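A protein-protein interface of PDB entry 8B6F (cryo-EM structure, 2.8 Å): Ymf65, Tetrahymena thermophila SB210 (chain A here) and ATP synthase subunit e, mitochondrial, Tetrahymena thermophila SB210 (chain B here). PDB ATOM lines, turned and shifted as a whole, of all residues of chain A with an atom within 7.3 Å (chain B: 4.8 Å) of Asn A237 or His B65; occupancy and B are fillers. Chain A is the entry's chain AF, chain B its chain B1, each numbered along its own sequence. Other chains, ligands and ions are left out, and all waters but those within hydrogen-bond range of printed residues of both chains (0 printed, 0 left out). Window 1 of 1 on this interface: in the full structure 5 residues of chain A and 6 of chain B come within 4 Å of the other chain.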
ATOM      1  N   ALA A 231      -2.570 -20.675  -4.438  1.00  0.00           N
ATOM      2  CA  ALA A 231      -2.411 -19.226  -4.489  1.00  0.00           C
ATOM      3  C   ALA A 231      -1.890 -18.777  -5.849  1.00  0.00           C
ATOM      4  O   ALA A 231      -2.369 -17.787  -6.411  1.00  0.00           O
ATOM      5  CB  ALA A 231      -1.479 -18.772  -3.370  1.00  0.00           C
ATOM      6  N   SER A 232      -0.909 -19.495  -6.394  1.00  0.00           N
ATOM      7  CA  SER A 232      -0.371 -19.148  -7.705  1.00  0.00           C
ATOM      8  C   SER A 232      -1.401 -19.357  -8.804  1.00  0.00           C
ATOM      9  O   SER A 232      -1.409 -18.620  -9.794  1.00  0.00           O
ATOM     10  CB  SER A 232       0.874 -19.971  -7.997  1.00  0.00           C
ATOM     11  OG  SER A 232       1.889 -19.729  -7.040  1.00  0.00           O
ATOM     12  N   ASN A 233      -2.266 -20.358  -8.648  1.00  0.00           N
ATOM     13  CA  ASN A 233      -3.353 -20.548  -9.598  1.00  0.00           C
ATOM     14  C   ASN A 233      -4.328 -19.382  -9.541  1.00  0.00           C
ATOM     15  O   ASN A 233      -4.813 -18.920 -10.579  1.00  0.00           O
ATOM     16  CB  ASN A 233      -4.068 -21.866  -9.310  1.00  0.00           C
ATOM     17  CG  ASN A 233      -5.270 -22.079 -10.196  1.00  0.00           C
ATOM     18  OD1 ASN A 233      -5.321 -21.587 -11.321  1.00  0.00           O
ATOM     19  ND2 ASN A 233      -6.255 -22.810  -9.689  1.00  0.00           N
ATOM     20  N   ASN A 234      -4.633 -18.896  -8.338  1.00  0.00           N
ATOM     21  CA  ASN A 234      -5.478 -17.714  -8.229  1.00  0.00           C
ATOM     22  C   ASN A 234      -4.819 -16.517  -8.900  1.00  0.00           C
ATOM     23  O   ASN A 234      -5.488 -15.727  -9.576  1.00  0.00           O
ATOM     24  CB  ASN A 234      -5.766 -17.410  -6.757  1.00  0.00           C
ATOM     25  CG  ASN A 234      -6.671 -18.443  -6.114  1.00  0.00           C
ATOM     26  OD1 ASN A 234      -7.452 -19.110  -6.791  1.00  0.00           O
ATOM     27  ND2 ASN A 234      -6.567 -18.581  -4.797  1.00  0.00           N
ATOM     28  N   GLN A 235      -3.505 -16.361  -8.720  1.00  0.00           N
ATOM     29  CA  GLN A 235      -2.803 -15.228  -9.317  1.00  0.00           C
ATOM     30  C   GLN A 235      -2.791 -15.329 -10.840  1.00  0.00           C
ATOM     31  O   GLN A 235      -3.143 -14.374 -11.539  1.00  0.00           O
ATOM     32  CB  GLN A 235      -1.375 -15.162  -8.770  1.00  0.00           C
ATOM     33  CG  GLN A 235      -0.553 -13.983  -9.270  1.00  0.00           C
ATOM     34  CD  GLN A 235      -1.077 -12.653  -8.774  1.00  0.00           C
ATOM     35  OE1 GLN A 235      -2.042 -12.596  -8.015  1.00  0.00           O
ATOM     36  NE2 GLN A 235      -0.438 -11.571  -9.200  1.00  0.00           N
ATOM     37  N   ILE A 236      -2.384 -16.485 -11.368  1.00  0.00           N
ATOM     38  CA  ILE A 236      -2.215 -16.632 -12.810  1.00  0.00           C
ATOM     39  C   ILE A 236      -3.558 -16.712 -13.519  1.00  0.00           C
ATOM     40  O   ILE A 236      -3.701 -16.232 -14.650  1.00  0.00           O
ATOM     41  CB  ILE A 236      -1.355 -17.875 -13.105  1.00  0.00           C
ATOM     42  CG1 ILE A 236       0.032 -17.721 -12.484  1.00  0.00           C
ATOM     43  CG2 ILE A 236      -1.230 -18.101 -14.606  1.00  0.00           C
ATOM     44  CD1 ILE A 236       0.754 -19.028 -12.309  1.00  0.00           C
ATOM     45  N   ASN A 237      -4.557 -17.324 -12.881  1.00  0.00           N
ATOM     46  CA  ASN A 237      -5.826 -17.650 -13.530  1.00  0.00           C
ATOM     47  C   ASN A 237      -5.625 -18.736 -14.586  1.00  0.00           C
ATOM     48  O   ASN A 237      -6.230 -18.700 -15.658  1.00  0.00           O
ATOM     49  CB  ASN A 237      -6.482 -16.410 -14.141  1.00  0.00           C
ATOM     50  CG  ASN A 237      -7.971 -16.583 -14.338  1.00  0.00           C
ATOM     51  OD1 ASN A 237      -8.533 -17.625 -14.007  1.00  0.00           O
ATOM     52  ND2 ASN A 237      -8.622 -15.558 -14.868  1.00  0.00           N
ATOM     53  N   TYR A 238      -4.766 -19.707 -14.277  1.00  0.00           N
ATOM     54  CA  TYR A 238      -4.498 -20.808 -15.195  1.00  0.00           C
ATOM     55  C   TYR A 238      -5.559 -21.896 -15.079  1.00  0.00           C
ATOM     56  O   TYR A 238      -6.271 -22.190 -16.045  1.00  0.00           O
ATOM     57  CB  TYR A 238      -3.104 -21.379 -14.919  1.00  0.00           C
ATOM     58  CG  TYR A 238      -2.799 -22.653 -15.667  1.00  0.00           C
ATOM     59  CD1 TYR A 238      -2.218 -22.618 -16.928  1.00  0.00           C
ATOM     60  CD2 TYR A 238      -3.084 -23.893 -15.110  1.00  0.00           C
ATOM     61  CE1 TYR A 238      -1.937 -23.779 -17.614  1.00  0.00           C
ATOM     62  CE2 TYR A 238      -2.805 -25.059 -15.787  1.00  0.00           C
ATOM     63  CZ  TYR A 238      -2.231 -24.995 -17.040  1.00  0.00           C
ATOM     64  OH  TYR A 238      -1.951 -26.153 -17.724  1.00  0.00           O
ATOM     65  N   TYR A 239      -5.677 -22.502 -13.902  1.00  0.00           N
ATOM     66  CA  TYR A 239      -6.645 -23.562 -13.646  1.00  0.00           C
ATOM     67  C   TYR A 239      -7.866 -22.928 -12.992  1.00  0.00           C
ATOM     68  O   TYR A 239      -7.783 -22.422 -11.869  1.00  0.00           O
ATOM     69  CB  TYR A 239      -6.030 -24.640 -12.755  1.00  0.00           C
ATOM     70  CG  TYR A 239      -6.869 -25.884 -12.610  1.00  0.00           C
ATOM     71  CD1 TYR A 239      -7.894 -25.949 -11.676  1.00  0.00           C
ATOM     72  CD2 TYR A 239      -6.624 -27.001 -13.394  1.00  0.00           C
ATOM     73  CE1 TYR A 239      -8.660 -27.089 -11.537  1.00  0.00           C
ATOM     74  CE2 TYR A 239      -7.384 -28.145 -13.263  1.00  0.00           C
ATOM     75  CZ  TYR A 239      -8.399 -28.183 -12.332  1.00  0.00           C
ATOM     76  OH  TYR A 239      -9.158 -29.322 -12.198  1.00  0.00           O
ATOM     77  N   THR A 240      -8.996 -22.955 -13.692  1.00  0.00           N
ATOM     78  CA  THR A 240     -10.198 -22.238 -13.279  1.00  0.00           C
ATOM     79  C   THR A 240     -11.427 -23.131 -13.380  1.00  0.00           C
ATOM     80  O   THR A 240     -12.466 -22.746 -13.919  1.00  0.00           O
ATOM     81  CB  THR A 240     -10.388 -20.974 -14.114  1.00  0.00           C
ATOM     82  OG1 THR A 240     -11.609 -20.325 -13.737  1.00  0.00           O
ATOM     83  CG2 THR A 240     -10.428 -21.310 -15.599  1.00  0.00           C
ATOM     84  N   ASN A 242     -13.872 -24.062 -11.199  1.00  0.00           N
ATOM     85  CA  ASN A 242     -14.529 -23.819  -9.922  1.00  0.00           C
ATOM     86  C   ASN A 242     -15.347 -25.023  -9.481  1.00  0.00           C
ATOM     87  O   ASN A 242     -15.463 -25.287  -8.280  1.00  0.00           O
ATOM     88  CB  ASN A 242     -15.419 -22.581 -10.018  1.00  0.00           C
ATOM     89  CG  ASN A 242     -14.643 -21.334 -10.388  1.00  0.00           C
ATOM     90  OD1 ASN A 242     -13.464 -21.202 -10.061  1.00  0.00           O
ATOM     91  ND2 ASN A 242     -15.302 -20.412 -11.075  1.00  0.00           N
ATOM     92  N   ASP B  58     -15.120 -14.360 -18.532  1.00  0.00           N
ATOM     93  CA  ASP B  58     -14.057 -15.202 -17.994  1.00  0.00           C
ATOM     94  C   ASP B  58     -12.798 -15.112 -18.846  1.00  0.00           C
ATOM     95  O   ASP B  58     -11.687 -15.015 -18.314  1.00  0.00           O
ATOM     96  CB  ASP B  58     -14.531 -16.651 -17.896  1.00  0.00           C
ATOM     97  CG  ASP B  58     -15.682 -16.821 -16.926  1.00  0.00           C
ATOM     98  OD1 ASP B  58     -15.745 -16.057 -15.940  1.00  0.00           O
ATOM     99  OD2 ASP B  58     -16.523 -17.717 -17.145  1.00  0.00           O
ATOM    100  N   VAL B  61     -11.115 -11.767 -18.266  1.00  0.00           N
ATOM    101  CA  VAL B  61     -10.405 -11.760 -16.991  1.00  0.00           C
ATOM    102  C   VAL B  61      -9.107 -12.549 -17.100  1.00  0.00           C
ATOM    103  O   VAL B  61      -8.064 -12.128 -16.585  1.00  0.00           O
ATOM    104  CB  VAL B  61     -11.313 -12.312 -15.875  1.00  0.00           C
ATOM    105  CG1 VAL B  61     -10.524 -12.523 -14.588  1.00  0.00           C
ATOM    106  CG2 VAL B  61     -12.474 -11.368 -15.630  1.00  0.00           C
ATOM    107  N   ARG B  62      -9.143 -13.699 -17.776  1.00  0.00           N
ATOM    108  CA  ARG B  62      -7.933 -14.500 -17.929  1.00  0.00           C
ATOM    109  C   ARG B  62      -6.864 -13.734 -18.694  1.00  0.00           C
ATOM    110  O   ARG B  62      -5.690 -13.738 -18.306  1.00  0.00           O
ATOM    111  CB  ARG B  62      -8.259 -15.813 -18.638  1.00  0.00           C
ATOM    112  CG  ARG B  62      -7.119 -16.818 -18.619  1.00  0.00           C
ATOM    113  CD  ARG B  62      -7.373 -17.971 -19.573  1.00  0.00           C
ATOM    114  NE  ARG B  62      -7.433 -17.516 -20.957  1.00  0.00           N
ATOM    115  CZ  ARG B  62      -6.372 -17.231 -21.698  1.00  0.00           C
ATOM    116  NH1 ARG B  62      -5.143 -17.334 -21.216  1.00  0.00           N
ATOM    117  NH2 ARG B  62      -6.546 -16.827 -22.952  1.00  0.00           N
ATOM    118  N   GLN B  63      -7.247 -13.071 -19.783  1.00  0.00           N
ATOM    119  CA  GLN B  63      -6.278 -12.296 -20.550  1.00  0.00           C
ATOM    120  C   GLN B  63      -5.747 -11.125 -19.734  1.00  0.00           C
ATOM    121  O   GLN B  63      -4.566 -10.778 -19.832  1.00  0.00           O
ATOM    122  CB  GLN B  63      -6.907 -11.820 -21.857  1.00  0.00           C
ATOM    123  CG  GLN B  63      -7.250 -12.964 -22.796  1.00  0.00           C
ATOM    124  CD  GLN B  63      -7.802 -12.489 -24.117  1.00  0.00           C
ATOM    125  OE1 GLN B  63      -8.076 -11.304 -24.300  1.00  0.00           O
ATOM    126  NE2 GLN B  63      -7.964 -13.414 -25.055  1.00  0.00           N
ATOM    127  N   TYR B  64      -6.607 -10.500 -18.926  1.00  0.00           N
ATOM    128  CA  TYR B  64      -6.143  -9.439 -18.040  1.00  0.00           C
ATOM    129  C   TYR B  64      -5.109  -9.969 -17.055  1.00  0.00           C
ATOM    130  O   TYR B  64      -4.079  -9.327 -16.818  1.00  0.00           O
ATOM    131  CB  TYR B  64      -7.320  -8.816 -17.295  1.00  0.00           C
ATOM    132  CG  TYR B  64      -6.903  -7.772 -16.289  1.00  0.00           C
ATOM    133  CD1 TYR B  64      -6.603  -6.478 -16.691  1.00  0.00           C
ATOM    134  CD2 TYR B  64      -6.811  -8.077 -14.938  1.00  0.00           C
ATOM    135  CE1 TYR B  64      -6.221  -5.518 -15.778  1.00  0.00           C
ATOM    136  CE2 TYR B  64      -6.430  -7.124 -14.017  1.00  0.00           C
ATOM    137  CZ  TYR B  64      -6.138  -5.847 -14.444  1.00  0.00           C
ATOM    138  OH  TYR B  64      -5.759  -4.893 -13.533  1.00  0.00           O
ATOM    139  N   HIS B  65      -5.368 -11.137 -16.465  1.00  0.00           N
ATOM    140  CA  HIS B  65      -4.398 -11.742 -15.560  1.00  0.00           C
ATOM    141  C   HIS B  65      -3.074 -11.979 -16.272  1.00  0.00           C
ATOM    142  O   HIS B  65      -2.002 -11.684 -15.734  1.00  0.00           O
ATOM    143  CB  HIS B  65      -4.945 -13.058 -15.004  1.00  0.00           C
ATOM    144  CG  HIS B  65      -5.867 -12.889 -13.837  1.00  0.00           C
ATOM    145  ND1 HIS B  65      -5.563 -13.359 -12.578  1.00  0.00           N
ATOM    146  CD2 HIS B  65      -7.089 -12.316 -13.738  1.00  0.00           C
ATOM    147  CE1 HIS B  65      -6.555 -13.078 -11.753  1.00  0.00           C
ATOM    148  NE2 HIS B  65      -7.494 -12.446 -12.432  1.00  0.00           N
ATOM    149  N   GLU B  66      -3.131 -12.521 -17.489  1.00  0.00           N
ATOM    150  CA  GLU B  66      -1.910 -12.815 -18.231  1.00  0.00           C
ATOM    151  C   GLU B  66      -1.101 -11.548 -18.485  1.00  0.00           C
ATOM    152  O   GLU B  66       0.103 -11.504 -18.214  1.00  0.00           O
ATOM    153  CB  GLU B  66      -2.262 -13.503 -19.550  1.00  0.00           C
ATOM    154  CG  GLU B  66      -1.058 -13.871 -20.400  1.00  0.00           C
ATOM    155  CD  GLU B  66      -1.451 -14.510 -21.718  1.00  0.00           C
ATOM    156  OE1 GLU B  66      -2.660 -14.530 -22.031  1.00  0.00           O
ATOM    157  OE2 GLU B  66      -0.554 -14.992 -22.440  1.00  0.00           O
ATOM    158  N   LYS B  67      -1.746 -10.508 -19.013  1.00  0.00           N
ATOM    159  CA  LYS B  67      -1.021  -9.281 -19.332  1.00  0.00           C
ATOM    160  C   LYS B  67      -0.484  -8.614 -18.073  1.00  0.00           C
ATOM    161  O   LYS B  67       0.629  -8.078 -18.076  1.00  0.00           O
ATOM    162  CB  LYS B  67      -1.918  -8.320 -20.110  1.00  0.00           C
ATOM    163  CG  LYS B  67      -3.123  -7.830 -19.334  1.00  0.00           C
ATOM    164  CD  LYS B  67      -4.019  -6.938 -20.185  1.00  0.00           C
ATOM    165  CE  LYS B  67      -3.335  -5.632 -20.563  1.00  0.00           C
ATOM    166  NZ  LYS B  67      -2.890  -4.856 -19.373  1.00  0.00           N
ATOM    167  N   THR B  68      -1.262  -8.627 -16.988  1.00  0.00           N
ATOM    168  CA  THR B  68      -0.800  -8.014 -15.748  1.00  0.00           C
ATOM    169  C   THR B  68       0.418  -8.741 -15.193  1.00  0.00           C
ATOM    170  O   THR B  68       1.380  -8.105 -14.750  1.00  0.00           O
ATOM    171  CB  THR B  68      -1.929  -8.002 -14.719  1.00  0.00           C
ATOM    172  OG1 THR B  68      -3.043  -7.265 -15.236  1.00  0.00           O
ATOM    173  CG2 THR B  68      -1.467  -7.362 -13.417  1.00  0.00           C
ATOM    174  N   ASN B  69       0.398 -10.075 -15.212  1.00  0.00           N
ATOM    175  CA  ASN B  69       1.556 -10.828 -14.743  1.00  0.00           C
ATOM    176  C   ASN B  69       2.772 -10.555 -15.616  1.00  0.00           C
ATOM    177  O   ASN B  69       3.890 -10.412 -15.110  1.00  0.00           O
ATOM    178  CB  ASN B  69       1.238 -12.322 -14.718  1.00  0.00           C
ATOM    179  CG  ASN B  69       0.162 -12.670 -13.712  1.00  0.00           C
ATOM    180  OD1 ASN B  69       0.098 -12.089 -12.630  1.00  0.00           O
ATOM    181  ND2 ASN B  69      -0.692 -13.619 -14.067  1.00  0.00           N
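O of Gln A235 is in hydrogen-bond range of ND1 of His B65.
N of Arg B62 lies close to ND2 of Asn A237 (3.5 Å).
NH1 of Arg B62 is in salt-bridge range of OE1 of Glu B66 (3.8 Å).
O of His B65 is in hydrogen-bond range of ND2 of Asn B69.
CE1 of His B65 touches O of Asn A234, 3.6 Å away.
Gln A235 touches Asn B69.
His B65 touches Ile A236 (CB to O, 3.4 Å).
CA of Ile A236 touches ND2 of Asn B69 (3.6 Å).
Asn A237 touches Val B61.
Asn A237 touches His B65.
Asn A237 touches three residues of chain B.
His B65 touches just these residues of chain A: Asn A234, Gln A235, Ile A236 and Asn A237.
Printed residues of chain A within 4 Å of Asn B69: Gln A235 (3.5 Å) and Ile A236 (3.6 Å).
Printed residues of chain A within 4 Å of Val B61: Asn A237 (3.6 Å).
Printed residues of chain B within 4 Å of Ile A236: His B65 (3.4 Å) and Asn B69 (3.6 Å).
Of the printed residues of chain A, Arg B62 touches Asn A237.
Printed residues of chain B within 4 Å of Asn A234: His B65 (3.6 Å).
Lys B67 touches none of the printed residues of chain A.
Tyr A239 touches none of the printed residues of chain B.
The nearest residue of chain B that does not touch Asn A237 is Asp B58 (4.6 Å).
The nearest residue of chain A that does not touch His B65 is Asn A233 (6.0 Å).
The nearest printed residue of chain B that does not touch Gln A235 is Thr B68 (6.0 Å).
Among the printed residues, 8 pairs touch across the chains.
Among the printed residues, no Asp or Glu carboxylate lies within 4 Å of a Lys or Arg side-chain nitrogen of the other chain.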
